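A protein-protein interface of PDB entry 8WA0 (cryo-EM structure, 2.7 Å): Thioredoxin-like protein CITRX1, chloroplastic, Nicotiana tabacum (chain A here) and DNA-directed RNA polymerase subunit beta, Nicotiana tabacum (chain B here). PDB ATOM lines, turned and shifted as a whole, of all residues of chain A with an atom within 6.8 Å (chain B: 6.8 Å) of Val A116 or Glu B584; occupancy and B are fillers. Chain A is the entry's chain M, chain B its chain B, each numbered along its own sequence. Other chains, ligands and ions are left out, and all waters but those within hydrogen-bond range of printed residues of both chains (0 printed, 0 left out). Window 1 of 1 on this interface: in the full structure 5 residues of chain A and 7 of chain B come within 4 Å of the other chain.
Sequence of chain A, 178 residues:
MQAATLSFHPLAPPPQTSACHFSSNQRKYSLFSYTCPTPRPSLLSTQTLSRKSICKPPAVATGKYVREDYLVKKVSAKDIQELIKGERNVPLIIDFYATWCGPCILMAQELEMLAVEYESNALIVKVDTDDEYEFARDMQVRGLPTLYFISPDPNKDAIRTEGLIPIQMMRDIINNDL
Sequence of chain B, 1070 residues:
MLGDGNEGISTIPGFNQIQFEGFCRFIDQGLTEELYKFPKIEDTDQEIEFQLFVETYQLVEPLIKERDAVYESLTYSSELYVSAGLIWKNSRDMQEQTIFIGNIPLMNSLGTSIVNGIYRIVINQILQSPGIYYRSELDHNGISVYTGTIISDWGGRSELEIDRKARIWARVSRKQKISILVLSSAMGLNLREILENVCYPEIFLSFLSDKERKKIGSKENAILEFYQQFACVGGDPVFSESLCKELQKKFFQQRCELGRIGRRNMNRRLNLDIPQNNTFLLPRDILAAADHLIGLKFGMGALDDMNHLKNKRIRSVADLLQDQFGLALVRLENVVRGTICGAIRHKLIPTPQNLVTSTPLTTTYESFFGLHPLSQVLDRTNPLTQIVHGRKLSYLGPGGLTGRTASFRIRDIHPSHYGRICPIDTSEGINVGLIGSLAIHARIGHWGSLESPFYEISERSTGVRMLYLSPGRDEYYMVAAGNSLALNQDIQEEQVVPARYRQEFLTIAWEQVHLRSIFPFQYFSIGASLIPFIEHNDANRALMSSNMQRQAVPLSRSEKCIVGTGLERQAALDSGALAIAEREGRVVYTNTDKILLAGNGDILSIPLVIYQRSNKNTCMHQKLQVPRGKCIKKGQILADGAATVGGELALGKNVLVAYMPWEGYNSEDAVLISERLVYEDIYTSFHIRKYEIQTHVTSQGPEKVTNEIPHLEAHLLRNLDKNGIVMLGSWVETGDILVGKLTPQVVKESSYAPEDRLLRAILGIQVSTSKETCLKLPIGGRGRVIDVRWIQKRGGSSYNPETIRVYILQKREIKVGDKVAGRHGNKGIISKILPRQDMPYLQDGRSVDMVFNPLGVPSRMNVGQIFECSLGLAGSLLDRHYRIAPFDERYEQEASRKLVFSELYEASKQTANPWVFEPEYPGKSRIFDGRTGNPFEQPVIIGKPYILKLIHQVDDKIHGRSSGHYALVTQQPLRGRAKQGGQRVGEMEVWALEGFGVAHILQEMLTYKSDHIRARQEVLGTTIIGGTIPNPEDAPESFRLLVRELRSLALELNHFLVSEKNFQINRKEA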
ATOM      1  N   ARG A  67       0.508   4.260   4.847  1.00  0.00           N
ATOM      2  CA  ARG A  67       1.655   4.545   4.053  1.00  0.00           C
ATOM      3  C   ARG A  67       2.130   3.319   3.352  1.00  0.00           C
ATOM      4  O   ARG A  67       2.159   2.248   3.927  1.00  0.00           O
ATOM      5  CB  ARG A  67       2.726   5.108   4.952  1.00  0.00           C
ATOM      6  CG  ARG A  67       4.100   5.330   4.354  1.00  0.00           C
ATOM      7  CD  ARG A  67       4.146   6.577   3.503  1.00  0.00           C
ATOM      8  NE  ARG A  67       5.515   6.899   3.135  1.00  0.00           N
ATOM      9  CZ  ARG A  67       5.847   7.835   2.257  1.00  0.00           C
ATOM     10  NH1 ARG A  67       4.902   8.534   1.650  1.00  0.00           N
ATOM     11  NH2 ARG A  67       7.122   8.063   1.980  1.00  0.00           N
ATOM     12  N   GLU A  68       2.506   3.457   2.103  1.00  0.00           N
ATOM     13  CA  GLU A  68       3.010   2.358   1.334  1.00  0.00           C
ATOM     14  C   GLU A  68       4.284   1.767   1.816  1.00  0.00           C
ATOM     15  O   GLU A  68       5.199   2.466   2.194  1.00  0.00           O
ATOM     16  CB  GLU A  68       3.235   2.851  -0.057  1.00  0.00           C
ATOM     17  CG  GLU A  68       2.012   3.470  -0.712  1.00  0.00           C
ATOM     18  CD  GLU A  68       1.980   4.984  -0.600  1.00  0.00           C
ATOM     19  OE1 GLU A  68       2.948   5.567  -0.066  1.00  0.00           O
ATOM     20  OE2 GLU A  68       0.985   5.591  -1.048  1.00  0.00           O
ATOM     21  N   LEU A  71       9.085   1.617  -1.417  1.00  0.00           N
ATOM     22  CA  LEU A  71       9.418   2.926  -1.913  1.00  0.00           C
ATOM     23  C   LEU A  71      10.231   3.039  -3.166  1.00  0.00           C
ATOM     24  O   LEU A  71      10.624   4.135  -3.508  1.00  0.00           O
ATOM     25  CB  LEU A  71      10.182   3.664  -0.825  1.00  0.00           C
ATOM     26  CG  LEU A  71       9.578   4.293   0.433  1.00  0.00           C
ATOM     27  CD1 LEU A  71       8.823   3.320   1.323  1.00  0.00           C
ATOM     28  CD2 LEU A  71      10.691   4.944   1.222  1.00  0.00           C
ATOM     29  N   LEU A 111      18.473  -1.806  -1.435  1.00  0.00           N
ATOM     30  CA  LEU A 111      18.042  -0.642  -2.163  1.00  0.00           C
ATOM     31  C   LEU A 111      16.932   0.085  -1.449  1.00  0.00           C
ATOM     32  O   LEU A 111      16.891   1.301  -1.475  1.00  0.00           O
ATOM     33  CB  LEU A 111      17.771  -0.970  -3.643  1.00  0.00           C
ATOM     34  CG  LEU A 111      18.906  -0.963  -4.659  1.00  0.00           C
ATOM     35  CD1 LEU A 111      19.446   0.436  -4.848  1.00  0.00           C
ATOM     36  CD2 LEU A 111      20.023  -1.878  -4.221  1.00  0.00           C
ATOM     37  N   GLU A 112      16.027  -0.618  -0.807  1.00  0.00           N
ATOM     38  CA  GLU A 112      15.022   0.036  -0.014  1.00  0.00           C
ATOM     39  C   GLU A 112      15.602   0.813   1.148  1.00  0.00           C
ATOM     40  O   GLU A 112      15.072   1.862   1.474  1.00  0.00           O
ATOM     41  CB  GLU A 112      13.865  -0.842   0.344  1.00  0.00           C
ATOM     42  CG  GLU A 112      12.795  -0.950  -0.719  1.00  0.00           C
ATOM     43  CD  GLU A 112      11.613  -1.769  -0.265  1.00  0.00           C
ATOM     44  OE1 GLU A 112      11.508  -2.940  -0.685  1.00  0.00           O
ATOM     45  OE2 GLU A 112      10.790  -1.248   0.517  1.00  0.00           O
ATOM     46  N   MET A 113      16.655   0.360   1.805  1.00  0.00           N
ATOM     47  CA  MET A 113      17.333   1.181   2.825  1.00  0.00           C
ATOM     48  C   MET A 113      18.024   2.428   2.347  1.00  0.00           C
ATOM     49  O   MET A 113      17.963   3.442   3.020  1.00  0.00           O
ATOM     50  CB  MET A 113      18.285   0.411   3.689  1.00  0.00           C
ATOM     51  CG  MET A 113      17.654  -0.264   4.881  1.00  0.00           C
ATOM     52  SD  MET A 113      17.479   0.894   6.241  1.00  0.00           S
ATOM     53  CE  MET A 113      19.183   1.373   6.483  1.00  0.00           C
ATOM     54  N   LEU A 114      18.667   2.400   1.206  1.00  0.00           N
ATOM     55  CA  LEU A 114      19.319   3.550   0.667  1.00  0.00           C
ATOM     56  C   LEU A 114      18.281   4.601   0.424  1.00  0.00           C
ATOM     57  O   LEU A 114      18.541   5.769   0.621  1.00  0.00           O
ATOM     58  CB  LEU A 114      20.130   3.190  -0.549  1.00  0.00           C
ATOM     59  CG  LEU A 114      21.390   3.895  -0.991  1.00  0.00           C
ATOM     60  CD1 LEU A 114      22.414   3.890   0.120  1.00  0.00           C
ATOM     61  CD2 LEU A 114      21.899   3.122  -2.188  1.00  0.00           C
ATOM     62  N   ALA A 115      17.106   4.220   0.027  1.00  0.00           N
ATOM     63  CA  ALA A 115      16.041   5.147  -0.170  1.00  0.00           C
ATOM     64  C   ALA A 115      15.585   5.884   1.033  1.00  0.00           C
ATOM     65  O   ALA A 115      15.321   7.062   0.951  1.00  0.00           O
ATOM     66  CB  ALA A 115      14.901   4.425  -0.767  1.00  0.00           C
ATOM     67  N   VAL A 116      15.480   5.228   2.164  1.00  0.00           N
ATOM     68  CA  VAL A 116      15.090   5.869   3.387  1.00  0.00           C
ATOM     69  C   VAL A 116      16.107   6.890   3.791  1.00  0.00           C
ATOM     70  O   VAL A 116      15.755   7.960   4.255  1.00  0.00           O
ATOM     71  CB  VAL A 116      14.737   4.858   4.477  1.00  0.00           C
ATOM     72  CG1 VAL A 116      14.295   5.553   5.748  1.00  0.00           C
ATOM     73  CG2 VAL A 116      13.660   3.911   3.992  1.00  0.00           C
ATOM     74  N   GLU A 117      17.361   6.603   3.626  1.00  0.00           N
ATOM     75  CA  GLU A 117      18.402   7.534   3.918  1.00  0.00           C
ATOM     76  C   GLU A 117      18.533   8.775   3.066  1.00  0.00           C
ATOM     77  O   GLU A 117      18.821   9.828   3.597  1.00  0.00           O
ATOM     78  CB  GLU A 117      19.690   6.762   3.897  1.00  0.00           C
ATOM     79  CG  GLU A 117      19.707   5.552   4.790  1.00  0.00           C
ATOM     80  CD  GLU A 117      21.002   4.801   4.673  1.00  0.00           C
ATOM     81  OE1 GLU A 117      21.810   5.166   3.799  1.00  0.00           O
ATOM     82  OE2 GLU A 117      21.214   3.851   5.446  1.00  0.00           O
ATOM     83  N   TYR A 118      18.327   8.699   1.775  1.00  0.00           N
ATOM     84  CA  TYR A 118      18.548   9.794   0.881  1.00  0.00           C
ATOM     85  C   TYR A 118      17.230  10.031   0.315  1.00  0.00           C
ATOM     86  O   TYR A 118      16.961   9.611  -0.797  1.00  0.00           O
ATOM     87  CB  TYR A 118      19.367   9.271  -0.265  1.00  0.00           C
ATOM     88  CG  TYR A 118      20.825   9.014  -0.084  1.00  0.00           C
ATOM     89  CD1 TYR A 118      21.727  10.048  -0.025  1.00  0.00           C
ATOM     90  CD2 TYR A 118      21.311   7.731  -0.076  1.00  0.00           C
ATOM     91  CE1 TYR A 118      23.073   9.806   0.105  1.00  0.00           C
ATOM     92  CE2 TYR A 118      22.651   7.481   0.054  1.00  0.00           C
ATOM     93  CZ  TYR A 118      23.524   8.523   0.141  1.00  0.00           C
ATOM     94  OH  TYR A 118      24.862   8.263   0.268  1.00  0.00           O
ATOM     95  N   GLU A 119      16.375  10.716   1.024  1.00  0.00           N
ATOM     96  CA  GLU A 119      15.010  10.844   0.604  1.00  0.00           C
ATOM     97  C   GLU A 119      14.599  11.593  -0.636  1.00  0.00           C
ATOM     98  O   GLU A 119      13.818  11.065  -1.413  1.00  0.00           O
ATOM     99  CB  GLU A 119      14.222  11.350   1.777  1.00  0.00           C
ATOM    100  CG  GLU A 119      14.837  12.541   2.495  1.00  0.00           C
ATOM    101  CD  GLU A 119      15.677  12.148   3.696  1.00  0.00           C
ATOM    102  OE1 GLU A 119      15.573  10.988   4.146  1.00  0.00           O
ATOM    103  OE2 GLU A 119      16.442  13.001   4.192  1.00  0.00           O
ATOM    104  N   ILE A 124      15.887   6.403  -6.918  1.00  0.00           N
ATOM    105  CA  ILE A 124      16.221   5.036  -7.131  1.00  0.00           C
ATOM    106  C   ILE A 124      15.068   4.419  -7.877  1.00  0.00           C
ATOM    107  O   ILE A 124      13.963   4.478  -7.404  1.00  0.00           O
ATOM    108  CB  ILE A 124      16.484   4.330  -5.809  1.00  0.00           C
ATOM    109  CG1 ILE A 124      17.546   5.066  -5.013  1.00  0.00           C
ATOM    110  CG2 ILE A 124      16.927   2.905  -6.057  1.00  0.00           C
ATOM    111  CD1 ILE A 124      17.921   4.381  -3.725  1.00  0.00           C
ATOM    112  N   ALA B 581       7.363   0.262  13.770  1.00  0.00           N
ATOM    113  CA  ALA B 581       7.163   1.496  13.044  1.00  0.00           C
ATOM    114  C   ALA B 581       5.999   1.542  12.146  1.00  0.00           C
ATOM    115  O   ALA B 581       5.676   0.579  11.503  1.00  0.00           O
ATOM    116  CB  ALA B 581       8.365   1.816  12.250  1.00  0.00           C
ATOM    117  N   GLU B 582       5.346   2.684  12.090  1.00  0.00           N
ATOM    118  CA  GLU B 582       4.186   2.845  11.263  1.00  0.00           C
ATOM    119  C   GLU B 582       4.476   3.589  10.007  1.00  0.00           C
ATOM    120  O   GLU B 582       3.620   3.704   9.162  1.00  0.00           O
ATOM    121  CB  GLU B 582       3.150   3.591  12.053  1.00  0.00           C
ATOM    122  CG  GLU B 582       1.744   3.036  11.925  1.00  0.00           C
ATOM    123  CD  GLU B 582       1.287   2.283  13.160  1.00  0.00           C
ATOM    124  OE1 GLU B 582       0.918   2.933  14.160  1.00  0.00           O
ATOM    125  OE2 GLU B 582       1.279   1.035  13.126  1.00  0.00           O
ATOM    126  N   ARG B 583       5.679   4.091   9.870  1.00  0.00           N
ATOM    127  CA  ARG B 583       6.057   4.851   8.737  1.00  0.00           C
ATOM    128  C   ARG B 583       7.551   4.733   8.726  1.00  0.00           C
ATOM    129  O   ARG B 583       8.113   4.368   9.710  1.00  0.00           O
ATOM    130  CB  ARG B 583       5.643   6.276   9.012  1.00  0.00           C
ATOM    131  CG  ARG B 583       5.923   7.249   7.892  1.00  0.00           C
ATOM    132  CD  ARG B 583       6.100   8.647   8.439  1.00  0.00           C
ATOM    133  NE  ARG B 583       4.887   9.111   9.095  1.00  0.00           N
ATOM    134  CZ  ARG B 583       3.928   9.799   8.488  1.00  0.00           C
ATOM    135  NH1 ARG B 583       4.040  10.111   7.204  1.00  0.00           N
ATOM    136  NH2 ARG B 583       2.862  10.181   9.169  1.00  0.00           N
ATOM    137  N   GLU B 584       8.217   4.990   7.626  1.00  0.00           N
ATOM    138  CA  GLU B 584       9.667   5.001   7.558  1.00  0.00           C
ATOM    139  C   GLU B 584      10.220   6.299   8.119  1.00  0.00           C
ATOM    140  O   GLU B 584       9.504   7.273   8.213  1.00  0.00           O
ATOM    141  CB  GLU B 584      10.087   4.825   6.110  1.00  0.00           C
ATOM    142  CG  GLU B 584      10.426   6.084   5.335  1.00  0.00           C
ATOM    143  CD  GLU B 584       9.219   6.749   4.710  1.00  0.00           C
ATOM    144  OE1 GLU B 584       8.127   6.156   4.729  1.00  0.00           O
ATOM    145  OE2 GLU B 584       9.362   7.871   4.190  1.00  0.00           O
ATOM    146  N   GLY B 585      11.482   6.343   8.521  1.00  0.00           N
ATOM    147  CA  GLY B 585      12.047   7.581   8.980  1.00  0.00           C
ATOM    148  C   GLY B 585      13.341   7.482   9.696  1.00  0.00           C
ATOM    149  O   GLY B 585      13.951   6.451   9.672  1.00  0.00           O
ATOM    150  N   ARG B 586      13.761   8.558  10.341  1.00  0.00           N
ATOM    151  CA  ARG B 586      14.998   8.590  11.093  1.00  0.00           C
ATOM    152  C   ARG B 586      14.659   8.988  12.500  1.00  0.00           C
ATOM    153  O   ARG B 586      13.768   9.766  12.691  1.00  0.00           O
ATOM    154  CB  ARG B 586      15.947   9.579  10.465  1.00  0.00           C
ATOM    155  CG  ARG B 586      17.340   9.612  11.043  1.00  0.00           C
ATOM    156  CD  ARG B 586      18.180  10.676  10.360  1.00  0.00           C
ATOM    157  NE  ARG B 586      19.103  10.116   9.379  1.00  0.00           N
ATOM    158  CZ  ARG B 586      18.907  10.116   8.065  1.00  0.00           C
ATOM    159  NH1 ARG B 586      17.813  10.657   7.549  1.00  0.00           N
ATOM    160  NH2 ARG B 586      19.813   9.580   7.264  1.00  0.00           N
ATOM    161  N   LEU B 597       9.908   9.858  15.491  1.00  0.00           N
ATOM    162  CA  LEU B 597      10.380   9.373  14.208  1.00  0.00           C
ATOM    163  C   LEU B 597      10.131  10.449  13.150  1.00  0.00           C
ATOM    164  O   LEU B 597       9.022  10.896  13.003  1.00  0.00           O
ATOM    165  CB  LEU B 597       9.575   8.130  13.855  1.00  0.00           C
ATOM    166  CG  LEU B 597      10.010   7.235  12.703  1.00  0.00           C
ATOM    167  CD1 LEU B 597      11.314   6.549  13.056  1.00  0.00           C
ATOM    168  CD2 LEU B 597       8.928   6.208  12.436  1.00  0.00           C
ATOM    169  N   ALA B 598      11.128  10.868  12.399  1.00  0.00           N
ATOM    170  CA  ALA B 598      10.925  11.950  11.459  1.00  0.00           C
ATOM    171  C   ALA B 598      11.046  11.563  10.053  1.00  0.00           C
ATOM    172  O   ALA B 598      12.137  11.497   9.532  1.00  0.00           O
ATOM    173  CB  ALA B 598      11.964  12.999  11.701  1.00  0.00           C
ATOM    174  N   GLY B 599       9.935  11.428   9.380  1.00  0.00           N
ATOM    175  CA  GLY B 599       9.980  10.962   8.022  1.00  0.00           C
ATOM    176  C   GLY B 599       9.403  11.899   7.019  1.00  0.00           C
ATOM    177  O   GLY B 599       8.263  12.302   7.194  1.00  0.00           O
ATOM    178  N   ASN B 600      10.137  12.253   5.968  1.00  0.00           N
ATOM    179  CA  ASN B 600       9.672  13.229   4.953  1.00  0.00           C
ATOM    180  C   ASN B 600       8.827  14.424   5.424  1.00  0.00           C
ATOM    181  O   ASN B 600       7.698  14.598   4.994  1.00  0.00           O
ATOM    182  CB  ASN B 600       9.051  12.547   3.695  1.00  0.00           C
ATOM    183  CG  ASN B 600       7.723  11.853   3.956  1.00  0.00           C
ATOM    184  OD1 ASN B 600       6.695  12.274   3.433  1.00  0.00           O
ATOM    185  ND2 ASN B 600       7.741  10.775   4.729  1.00  0.00           N
ATOM    186  N   CYS B 631      18.012   5.024  10.643  1.00  0.00           N
ATOM    187  CA  CYS B 631      16.934   4.880   9.700  1.00  0.00           C
ATOM    188  C   CYS B 631      16.146   3.616   9.909  1.00  0.00           C
ATOM    189  O   CYS B 631      16.703   2.600  10.232  1.00  0.00           O
ATOM    190  CB  CYS B 631      17.469   4.991   8.303  1.00  0.00           C
ATOM    191  SG  CYS B 631      18.323   6.533   8.014  1.00  0.00           S
ATOM    192  N   ILE B 632      14.848   3.672   9.713  1.00  0.00           N
ATOM    193  CA  ILE B 632      14.007   2.562   9.963  1.00  0.00           C
ATOM    194  C   ILE B 632      13.084   2.430   8.784  1.00  0.00           C
ATOM    195  O   ILE B 632      12.822   3.394   8.140  1.00  0.00           O
ATOM    196  CB  ILE B 632      13.252   2.806  11.294  1.00  0.00           C
ATOM    197  CG1 ILE B 632      13.299   1.578  12.195  1.00  0.00           C
ATOM    198  CG2 ILE B 632      11.812   3.221  11.069  1.00  0.00           C
ATOM    199  CD1 ILE B 632      14.617   1.399  12.904  1.00  0.00           C
ATOM    200  N   LYS B 633      12.610   1.245   8.467  1.00  0.00           N
ATOM    201  CA  LYS B 633      11.680   1.022   7.405  1.00  0.00           C
ATOM    202  C   LYS B 633      10.436   0.616   8.092  1.00  0.00           C
ATOM    203  O   LYS B 633      10.483   0.273   9.226  1.00  0.00           O
ATOM    204  CB  LYS B 633      12.138  -0.108   6.542  1.00  0.00           C
ATOM    205  CG  LYS B 633      13.423   0.124   5.803  1.00  0.00           C
ATOM    206  CD  LYS B 633      13.565  -0.843   4.644  1.00  0.00           C
ATOM    207  CE  LYS B 633      13.719  -2.276   5.106  1.00  0.00           C
ATOM    208  NZ  LYS B 633      14.149  -3.171   4.002  1.00  0.00           N
ATOM    209  N   LYS B 634       9.300   0.712   7.452  1.00  0.00           N
ATOM    210  CA  LYS B 634       8.038   0.395   8.061  1.00  0.00           C
ATOM    211  C   LYS B 634       8.006  -1.033   8.444  1.00  0.00           C
ATOM    212  O   LYS B 634       8.318  -1.872   7.654  1.00  0.00           O
ATOM    213  CB  LYS B 634       6.927   0.685   7.083  1.00  0.00           C
ATOM    214  CG  LYS B 634       5.525   0.485   7.578  1.00  0.00           C
ATOM    215  CD  LYS B 634       4.560   1.005   6.545  1.00  0.00           C
ATOM    216  CE  LYS B 634       3.135   0.871   7.023  1.00  0.00           C
ATOM    217  NZ  LYS B 634       2.651  -0.528   6.993  1.00  0.00           N
ATOM    218  N   GLY B 635       7.556  -1.333   9.638  1.00  0.00           N
ATOM    219  CA  GLY B 635       7.495  -2.674  10.125  1.00  0.00           C
ATOM    220  C   GLY B 635       8.640  -3.136  10.940  1.00  0.00           C
ATOM    221  O   GLY B 635       8.593  -4.212  11.451  1.00  0.00           O
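The guanidinium group (NE) of Arg A67 lies within salt-bridge range of the side-chain carboxylate (OE1) of Glu B584, 3.1 Å away.
NH1 of Arg A67 is in salt-bridge range of OE1 of Glu A68. The side-chain carboxylate of Glu B584 lies within hydrogen-bond range of the side-chain amide nitrogen of Asn B600, 3.4 Å away. O of Gly B585 sits at hydrogen-bond distance from N of Ile B632 (2.9 Å). O of Arg B586 lies within hydrogen-bond range of N of Ala B598, at 2.9 Å. The side-chain sulfur (SG) of Cys B631 sits at hydrogen-bond distance from the guanidinium group (NH2) of Arg B586.
Among the printed residues, merely in contact across the chains: Arg A67 with Asn B600 (3.9 Å), Arg A67 with Lys B634 (3.5 Å), Val A116 with Glu B584 (3.9 Å), Val A116 with Ile B632 (3.5 Å), Glu A117 with Arg B586 (3.8 Å) and Glu A117 with Cys B631 (3.6 Å).
Val A116 touches two residues of chain B. Of chain A, only Arg A67 (3.1 Å) and Val A116 (3.9 Å) come within 4 Å of Glu B584. Printed residues of chain A within 4 Å of Cys B631: Glu A117. Printed residues of chain A within 4 Å of Arg B586: Glu A117. Of the printed residues of chain A, Ile B632 touches Val A116 (3.5 Å). Glu A68 touches none of the printed residues of chain B. The nearest residue of chain A that does not touch Glu B584 is Leu A71 (4.2 Å). The nearest printed residue of chain A that does not touch Lys B634 is Glu A68 (4.6 Å).
Of the 13 printed residues of chain A, 3 touch a printed residue of chain B. Hydrophobic or aromatic side chains of chain A within 4 Å of the printed part of chain B: Val A116. Among the printed residues, 7 pairs touch across the chains. Among the printed residues, Asp or Glu carboxylates within 4 Å of a Lys or Arg side-chain nitrogen of the other chain: Arg A67 with Glu B584.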
